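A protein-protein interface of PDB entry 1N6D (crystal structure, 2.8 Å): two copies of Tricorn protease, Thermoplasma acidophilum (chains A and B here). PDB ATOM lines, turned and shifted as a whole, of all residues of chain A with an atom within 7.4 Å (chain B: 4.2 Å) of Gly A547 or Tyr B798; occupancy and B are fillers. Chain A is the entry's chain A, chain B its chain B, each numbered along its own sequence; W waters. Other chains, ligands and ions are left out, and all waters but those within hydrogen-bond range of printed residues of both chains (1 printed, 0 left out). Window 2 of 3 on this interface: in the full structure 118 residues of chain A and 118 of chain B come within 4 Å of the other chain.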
ATOM      1  N   PRO A 543      -3.466  17.347 -10.292  1.00  0.00           N
ATOM      2  CA  PRO A 543      -3.927  17.815  -8.982  1.00  0.00           C
ATOM      3  C   PRO A 543      -5.118  16.957  -8.580  1.00  0.00           C
ATOM      4  O   PRO A 543      -6.029  16.713  -9.373  1.00  0.00           O
ATOM      5  CB  PRO A 543      -4.302  19.276  -9.238  1.00  0.00           C
ATOM      6  CG  PRO A 543      -4.661  19.286 -10.683  1.00  0.00           C
ATOM      7  CD  PRO A 543      -3.596  18.412 -11.297  1.00  0.00           C
ATOM      8  N   LEU A 544      -5.088  16.473  -7.348  1.00  0.00           N
ATOM      9  CA  LEU A 544      -6.131  15.602  -6.813  1.00  0.00           C
ATOM     10  C   LEU A 544      -7.420  16.360  -6.481  1.00  0.00           C
ATOM     11  O   LEU A 544      -8.434  15.746  -6.151  1.00  0.00           O
ATOM     12  CB  LEU A 544      -5.588  14.921  -5.564  1.00  0.00           C
ATOM     13  CG  LEU A 544      -4.218  14.280  -5.753  1.00  0.00           C
ATOM     14  CD1 LEU A 544      -3.767  13.598  -4.450  1.00  0.00           C
ATOM     15  CD2 LEU A 544      -4.301  13.279  -6.887  1.00  0.00           C
ATOM     16  N   ILE A 545      -7.350  17.686  -6.561  1.00  0.00           N
ATOM     17  CA  ILE A 545      -8.476  18.552  -6.305  1.00  0.00           C
ATOM     18  C   ILE A 545      -8.866  19.341  -7.549  1.00  0.00           C
ATOM     19  O   ILE A 545      -8.205  20.322  -7.909  1.00  0.00           O
ATOM     20  CB  ILE A 545      -8.159  19.584  -5.212  1.00  0.00           C
ATOM     21  CG1 ILE A 545      -7.838  18.892  -3.916  1.00  0.00           C
ATOM     22  CG2 ILE A 545      -9.331  20.532  -5.031  1.00  0.00           C
ATOM     23  CD1 ILE A 545      -7.498  19.904  -2.829  1.00  0.00           C
ATOM     24  N   PRO A 546      -9.938  18.926  -8.220  1.00  0.00           N
ATOM     25  CA  PRO A 546     -10.418  19.601  -9.421  1.00  0.00           C
ATOM     26  C   PRO A 546     -10.496  21.094  -9.199  1.00  0.00           C
ATOM     27  O   PRO A 546     -10.943  21.533  -8.138  1.00  0.00           O
ATOM     28  CB  PRO A 546     -11.794  18.997  -9.622  1.00  0.00           C
ATOM     29  CG  PRO A 546     -11.622  17.617  -9.128  1.00  0.00           C
ATOM     30  CD  PRO A 546     -10.824  17.814  -7.852  1.00  0.00           C
ATOM     31  N   GLY A 547     -10.074  21.865 -10.202  1.00  0.00           N
ATOM     32  CA  GLY A 547     -10.116  23.320 -10.110  1.00  0.00           C
ATOM     33  C   GLY A 547      -8.740  23.892  -9.844  1.00  0.00           C
ATOM     34  O   GLY A 547      -8.442  25.019 -10.228  1.00  0.00           O
ATOM     35  N   SER A 548      -7.894  23.103  -9.194  1.00  0.00           N
ATOM     36  CA  SER A 548      -6.554  23.545  -8.880  1.00  0.00           C
ATOM     37  C   SER A 548      -5.700  23.414 -10.138  1.00  0.00           C
ATOM     38  O   SER A 548      -5.774  22.414 -10.848  1.00  0.00           O
ATOM     39  CB  SER A 548      -6.012  22.709  -7.727  1.00  0.00           C
ATOM     40  OG  SER A 548      -4.676  23.089  -7.435  1.00  0.00           O
ATOM     41  N   PRO A 549      -4.902  24.445 -10.449  1.00  0.00           N
ATOM     42  CA  PRO A 549      -4.056  24.416 -11.640  1.00  0.00           C
ATOM     43  C   PRO A 549      -2.759  23.653 -11.434  1.00  0.00           C
ATOM     44  O   PRO A 549      -2.488  23.127 -10.346  1.00  0.00           O
ATOM     45  CB  PRO A 549      -3.813  25.893 -11.917  1.00  0.00           C
ATOM     46  CG  PRO A 549      -3.736  26.463 -10.541  1.00  0.00           C
ATOM     47  CD  PRO A 549      -4.894  25.786  -9.840  1.00  0.00           C
ATOM     48  N   ASN A 550      -1.973  23.577 -12.501  1.00  0.00           N
ATOM     49  CA  ASN A 550      -0.691  22.912 -12.470  1.00  0.00           C
ATOM     50  C   ASN A 550       0.197  23.745 -11.561  1.00  0.00           C
ATOM     51  O   ASN A 550       0.534  24.894 -11.862  1.00  0.00           O
ATOM     52  CB  ASN A 550      -0.097  22.874 -13.885  1.00  0.00           C
ATOM     53  CG  ASN A 550       1.195  22.085 -13.959  1.00  0.00           C
ATOM     54  OD1 ASN A 550       1.999  22.090 -13.008  1.00  0.00           O
ATOM     55  ND2 ASN A 550       1.414  21.411 -15.086  1.00  0.00           N
ATOM     56  N   LYS A 553       2.896  25.831 -13.039  1.00  0.00           N
ATOM     57  CA  LYS A 553       2.541  26.949 -13.899  1.00  0.00           C
ATOM     58  C   LYS A 553       2.604  28.295 -13.185  1.00  0.00           C
ATOM     59  O   LYS A 553       2.401  29.340 -13.800  1.00  0.00           O
ATOM     60  CB  LYS A 553       1.153  26.747 -14.496  1.00  0.00           C
ATOM     61  CG  LYS A 553       1.136  25.729 -15.626  1.00  0.00           C
ATOM     62  CD  LYS A 553      -0.165  25.839 -16.399  1.00  0.00           C
ATOM     63  CE  LYS A 553      -0.147  25.006 -17.643  1.00  0.00           C
ATOM     64  NZ  LYS A 553      -1.341  25.292 -18.447  1.00  0.00           N
ATOM     65  N   VAL A 555       0.610  29.915 -11.169  1.00  0.00           N
ATOM     66  CA  VAL A 555      -0.578  30.740 -11.325  1.00  0.00           C
ATOM     67  C   VAL A 555      -0.855  31.479 -10.024  1.00  0.00           C
ATOM     68  O   VAL A 555      -1.182  30.848  -9.022  1.00  0.00           O
ATOM     69  CB  VAL A 555      -1.811  29.886 -11.682  1.00  0.00           C
ATOM     70  CG1 VAL A 555      -3.037  30.784 -11.844  1.00  0.00           C
ATOM     71  CG2 VAL A 555      -1.555  29.128 -12.959  1.00  0.00           C
ATOM     72  N   MET A 559      -5.456  34.866  -8.204  1.00  0.00           N
ATOM     73  CA  MET A 559      -6.184  34.652  -9.448  1.00  0.00           C
ATOM     74  C   MET A 559      -6.752  33.248  -9.614  1.00  0.00           C
ATOM     75  O   MET A 559      -7.231  32.888 -10.691  1.00  0.00           O
ATOM     76  CB  MET A 559      -5.279  34.996 -10.627  1.00  0.00           C
ATOM     77  CG  MET A 559      -4.881  36.451 -10.665  1.00  0.00           C
ATOM     78  SD  MET A 559      -3.698  36.747 -11.962  1.00  0.00           S
ATOM     79  CE  MET A 559      -2.874  38.208 -11.395  1.00  0.00           C
ATOM     80  N   THR A 560      -6.672  32.451  -8.553  1.00  0.00           N
ATOM     81  CA  THR A 560      -7.215  31.091  -8.560  1.00  0.00           C
ATOM     82  C   THR A 560      -8.011  30.875  -7.283  1.00  0.00           C
ATOM     83  O   THR A 560      -7.913  31.647  -6.320  1.00  0.00           O
ATOM     84  CB  THR A 560      -6.121  29.998  -8.654  1.00  0.00           C
ATOM     85  OG1 THR A 560      -4.953  30.411  -7.932  1.00  0.00           O
ATOM     86  CG2 THR A 560      -5.784  29.726 -10.105  1.00  0.00           C
ATOM     87  N   SER A 561      -8.815  29.825  -7.278  1.00  0.00           N
ATOM     88  CA  SER A 561      -9.638  29.515  -6.122  1.00  0.00           C
ATOM     89  C   SER A 561      -9.551  28.038  -5.805  1.00  0.00           C
ATOM     90  O   SER A 561     -10.532  27.313  -5.953  1.00  0.00           O
ATOM     91  CB  SER A 561     -11.086  29.908  -6.409  1.00  0.00           C
ATOM     92  OG  SER A 561     -11.510  29.378  -7.656  1.00  0.00           O
ATOM     93  N   GLU A 562      -8.378  27.587  -5.366  1.00  0.00           N
ATOM     94  CA  GLU A 562      -8.200  26.170  -5.032  1.00  0.00           C
ATOM     95  C   GLU A 562      -8.996  25.808  -3.774  1.00  0.00           C
ATOM     96  O   GLU A 562     -10.134  26.249  -3.589  1.00  0.00           O
ATOM     97  CB  GLU A 562      -6.716  25.831  -4.814  1.00  0.00           C
ATOM     98  N   ALA A 563      -8.397  24.982  -2.927  1.00  0.00           N
ATOM     99  CA  ALA A 563      -9.034  24.573  -1.691  1.00  0.00           C
ATOM    100  C   ALA A 563     -10.408  23.947  -1.909  1.00  0.00           C
ATOM    101  O   ALA A 563     -11.356  24.229  -1.170  1.00  0.00           O
ATOM    102  CB  ALA A 563      -9.146  25.773  -0.738  1.00  0.00           C
ATOM    103  N   GLY A 564     -10.521  23.119  -2.940  1.00  0.00           N
ATOM    104  CA  GLY A 564     -11.777  22.441  -3.194  1.00  0.00           C
ATOM    105  C   GLY A 564     -11.810  21.195  -2.314  1.00  0.00           C
ATOM    106  O   GLY A 564     -11.763  21.289  -1.085  1.00  0.00           O
ATOM    107  N   LYS A 573      -8.200  13.693 -17.091  1.00  0.00           N
ATOM    108  CA  LYS A 573      -8.561  14.778 -17.989  1.00  0.00           C
ATOM    109  C   LYS A 573      -7.893  16.072 -17.553  1.00  0.00           C
ATOM    110  O   LYS A 573      -7.600  16.925 -18.387  1.00  0.00           O
ATOM    111  CB  LYS A 573     -10.073  14.978 -18.018  1.00  0.00           C
ATOM    112  CG  LYS A 573     -10.825  13.820 -18.647  1.00  0.00           C
ATOM    113  CD  LYS A 573     -12.292  14.151 -18.798  1.00  0.00           C
ATOM    114  CE  LYS A 573     -13.041  13.000 -19.421  1.00  0.00           C
ATOM    115  NZ  LYS A 573     -14.482  13.329 -19.586  1.00  0.00           N
ATOM    116  N   ARG A 574      -7.651  16.207 -16.249  1.00  0.00           N
ATOM    117  CA  ARG A 574      -7.030  17.399 -15.672  1.00  0.00           C
ATOM    118  C   ARG A 574      -5.523  17.325 -15.787  1.00  0.00           C
ATOM    119  O   ARG A 574      -4.815  18.270 -15.405  1.00  0.00           O
ATOM    120  CB  ARG A 574      -7.368  17.519 -14.187  1.00  0.00           C
ATOM    121  CG  ARG A 574      -8.777  17.114 -13.807  1.00  0.00           C
ATOM    122  CD  ARG A 574      -9.163  17.682 -12.420  1.00  0.00           C
ATOM    123  NE  ARG A 574      -8.553  17.002 -11.283  1.00  0.00           N
ATOM    124  CZ  ARG A 574      -8.998  15.870 -10.743  1.00  0.00           C
ATOM    125  NH1 ARG A 574      -8.363  15.338  -9.704  1.00  0.00           N
ATOM    126  NH2 ARG A 574     -10.075  15.273 -11.225  1.00  0.00           N
ATOM    127  N   SER A 575      -5.020  16.198 -16.285  1.00  0.00           N
ATOM    128  CA  SER A 575      -3.573  16.038 -16.406  1.00  0.00           C
ATOM    129  C   SER A 575      -2.948  17.187 -17.190  1.00  0.00           C
ATOM    130  O   SER A 575      -3.566  17.756 -18.089  1.00  0.00           O
ATOM    131  CB  SER A 575      -3.221  14.720 -17.088  1.00  0.00           C
ATOM    132  OG  SER A 575      -3.540  14.791 -18.471  1.00  0.00           O
ATOM    133  N   ILE B 795      -9.326  23.955 -21.277  1.00  0.00           N
ATOM    134  CA  ILE B 795     -10.328  24.047 -20.213  1.00  0.00           C
ATOM    135  C   ILE B 795     -10.394  22.720 -19.439  1.00  0.00           C
ATOM    136  O   ILE B 795     -10.626  22.714 -18.219  1.00  0.00           O
ATOM    137  CB  ILE B 795     -11.722  24.407 -20.769  1.00  0.00           C
ATOM    138  CG1 ILE B 795     -11.736  25.893 -21.151  1.00  0.00           C
ATOM    139  CG2 ILE B 795     -12.809  24.146 -19.728  1.00  0.00           C
ATOM    140  CD1 ILE B 795     -13.048  26.391 -21.730  1.00  0.00           C
ATOM    141  N   PHE B 796     -10.158  21.603 -20.137  1.00  0.00           N
ATOM    142  CA  PHE B 796     -10.198  20.293 -19.498  1.00  0.00           C
ATOM    143  C   PHE B 796      -9.329  20.177 -18.243  1.00  0.00           C
ATOM    144  O   PHE B 796      -9.687  19.450 -17.311  1.00  0.00           O
ATOM    145  CB  PHE B 796      -9.818  19.189 -20.484  1.00  0.00           C
ATOM    146  CG  PHE B 796     -10.905  18.847 -21.463  1.00  0.00           C
ATOM    147  CD1 PHE B 796     -10.822  19.254 -22.788  1.00  0.00           C
ATOM    148  CD2 PHE B 796     -11.989  18.072 -21.069  1.00  0.00           C
ATOM    149  CE1 PHE B 796     -11.799  18.887 -23.704  1.00  0.00           C
ATOM    150  CE2 PHE B 796     -12.967  17.700 -21.968  1.00  0.00           C
ATOM    151  CZ  PHE B 796     -12.875  18.105 -23.291  1.00  0.00           C
ATOM    152  N   GLU B 797      -8.210  20.900 -18.195  1.00  0.00           N
ATOM    153  CA  GLU B 797      -7.329  20.826 -17.036  1.00  0.00           C
ATOM    154  C   GLU B 797      -8.035  21.165 -15.747  1.00  0.00           C
ATOM    155  O   GLU B 797      -7.583  20.763 -14.675  1.00  0.00           O
ATOM    156  CB  GLU B 797      -6.114  21.735 -17.207  1.00  0.00           C
ATOM    157  CG  GLU B 797      -5.188  21.309 -18.323  1.00  0.00           C
ATOM    158  CD  GLU B 797      -3.776  21.852 -18.143  1.00  0.00           C
ATOM    159  OE1 GLU B 797      -2.947  21.702 -19.058  1.00  0.00           O
ATOM    160  OE2 GLU B 797      -3.500  22.429 -17.076  1.00  0.00           O
ATOM    161  N   TYR B 798      -9.150  21.892 -15.838  1.00  0.00           N
ATOM    162  CA  TYR B 798      -9.918  22.269 -14.643  1.00  0.00           C
ATOM    163  C   TYR B 798     -11.004  21.259 -14.343  1.00  0.00           C
ATOM    164  O   TYR B 798     -11.935  21.553 -13.605  1.00  0.00           O
ATOM    165  CB  TYR B 798     -10.531  23.664 -14.817  1.00  0.00           C
ATOM    166  CG  TYR B 798      -9.517  24.772 -14.719  1.00  0.00           C
ATOM    167  CD1 TYR B 798      -8.633  25.022 -15.761  1.00  0.00           C
ATOM    168  CD2 TYR B 798      -9.381  25.513 -13.548  1.00  0.00           C
ATOM    169  CE1 TYR B 798      -7.634  25.972 -15.642  1.00  0.00           C
ATOM    170  CE2 TYR B 798      -8.381  26.458 -13.422  1.00  0.00           C
ATOM    171  CZ  TYR B 798      -7.511  26.682 -14.473  1.00  0.00           C
ATOM    172  OH  TYR B 798      -6.500  27.598 -14.355  1.00  0.00           O
ATOM    173  N   GLY B 799     -10.871  20.068 -14.917  1.00  0.00           N
ATOM    174  CA  GLY B 799     -11.842  19.019 -14.678  1.00  0.00           C
ATOM    175  C   GLY B 799     -13.272  19.354 -15.052  1.00  0.00           C
ATOM    176  O   GLY B 799     -14.161  19.197 -14.225  1.00  0.00           O
ATOM    177  N   ILE B 800     -13.493  19.818 -16.281  1.00  0.00           N
ATOM    178  CA  ILE B 800     -14.835  20.152 -16.770  1.00  0.00           C
ATOM    179  C   ILE B 800     -14.848  20.226 -18.284  1.00  0.00           C
ATOM    180  O   ILE B 800     -13.999  20.887 -18.873  1.00  0.00           O
ATOM    181  CB  ILE B 800     -15.334  21.511 -16.239  1.00  0.00           C
ATOM    182  CG1 ILE B 800     -14.178  22.512 -16.228  1.00  0.00           C
ATOM    183  CG2 ILE B 800     -15.977  21.348 -14.865  1.00  0.00           C
ATOM    184  CD1 ILE B 800     -14.500  23.821 -15.512  1.00  0.00           C
ATOM    185  N   LEU B 847     -12.291  30.317 -14.648  1.00  0.00           N
ATOM    186  CA  LEU B 847     -10.928  29.818 -14.714  1.00  0.00           C
ATOM    187  C   LEU B 847      -9.929  30.620 -15.555  1.00  0.00           C
ATOM    188  O   LEU B 847     -10.318  31.362 -16.451  1.00  0.00           O
ATOM    189  CB  LEU B 847     -10.962  28.384 -15.230  1.00  0.00           C
ATOM    190  CG  LEU B 847     -12.359  27.844 -15.466  1.00  0.00           C
ATOM    191  CD1 LEU B 847     -12.277  26.584 -16.296  1.00  0.00           C
ATOM    192  CD2 LEU B 847     -13.048  27.576 -14.128  1.00  0.00           C
ATOM    193  N   MET B 848      -8.640  30.466 -15.238  1.00  0.00           N
ATOM    194  CA  MET B 848      -7.561  31.115 -15.982  1.00  0.00           C
ATOM    195  C   MET B 848      -7.164  30.134 -17.074  1.00  0.00           C
ATOM    196  O   MET B 848      -6.462  29.153 -16.821  1.00  0.00           O
ATOM    197  CB  MET B 848      -6.344  31.384 -15.106  1.00  0.00           C
ATOM    198  CG  MET B 848      -6.474  32.565 -14.160  1.00  0.00           C
ATOM    199  SD  MET B 848      -6.644  34.185 -14.963  1.00  0.00           S
ATOM    200  CE  MET B 848      -4.947  34.600 -15.277  1.00  0.00           C
ATOM    201  N   ILE B 849      -7.613  30.416 -18.291  1.00  0.00           N
ATOM    202  CA  ILE B 849      -7.357  29.554 -19.432  1.00  0.00           C
ATOM    203  C   ILE B 849      -6.177  30.024 -20.258  1.00  0.00           C
ATOM    204  O   ILE B 849      -5.913  31.209 -20.390  1.00  0.00           O
ATOM    205  CB  ILE B 849      -8.594  29.490 -20.325  1.00  0.00           C
ATOM    206  CG1 ILE B 849      -9.792  29.042 -19.494  1.00  0.00           C
ATOM    207  CG2 ILE B 849      -8.341  28.562 -21.482  1.00  0.00           C
ATOM    208  CD1 ILE B 849      -9.548  27.787 -18.726  1.00  0.00           C
HETATM  209  O   HOH W   1      -7.515  21.011 -12.253  1.00  0.00           O
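Of the 19 printed residues of chain A, 6 touch a printed residue of chain B. Printed residues of chain A that touch a printed residue of chain B: Gly A547, Lys A553, Met A559, Lys A573, Arg A574 and Ser A575. Printed residues of chain B that touch a printed residue of chain A: Phe B796, Glu B797, Tyr B798, Gly B799 and Met B848. Hydrophobic or aromatic side chains of chain B within 4 Å of the printed part of chain A: Phe B796, Tyr B798 and Met B848. Along chain B the printed residues that touch a printed residue of chain A span positions 796 to 848. Among the printed residues, Asp or Glu carboxylates within 4 Å of a Lys or Arg side-chain nitrogen of the other chain: Lys A553 with Glu B797.
O of Lys A573 lies close to O of Phe B796, at 3.4 Å. The side-chain carboxylate (OE2) of Glu B797 is in salt-bridge range of the side-chain amino group (NZ) of Lys A553, at 3.8 Å.
O of Pro A543 lies within hydrogen-bond range of NH1 of Arg A574. The backbone carbonyl oxygen (O) of Met B848 lies within hydrogen-bond range of the side-chain hydroxyl (OH) of Tyr B798, at 2.9 Å.
Water W1 lies within hydrogen-bond range of the backbone carbonyl oxygen (O) of Glu B797, the backbone carbonyl oxygen (O) of Ser A548 and the backbone NH (N) of Gly A547.
Of chain B, only Tyr B798 (3.5 Å) comes within 4 Å of Gly A547. Of the printed residues of chain A, Tyr B798 touches Gly A547 (3.5 Å). Of chain A, only Arg A574 comes within 4 Å of Gly B799. Of the printed residues of chain B, Lys A553 touches Glu B797. Of the printed residues of chain A, Phe B796 touches Lys A573 and Arg A574. Of the printed residues of chain B, Lys A573 touches Phe B796. Of the printed residues of chain B, Arg A574 touches Phe B796 (3.7 Å), Glu B797 (3.3 Å) and Gly B799 (3.7 Å). Ile A545 touches none of the printed residues of chain B. The nearest printed residue of chain B that does not touch Gly A547 is Gly B799 (5.1 Å). The nearest printed residue of chain B that does not touch Lys A553 is Met B848 (6.6 Å).
Among the printed residues, merely in contact across the chains: Arg A574 with Glu B797, Gly A547 with Tyr B798, Met A559 with Met B848, Arg A574 with Gly B799, Arg A574 with Phe B796 and Ser A575 with Glu B797.
No position is printed for both chains.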
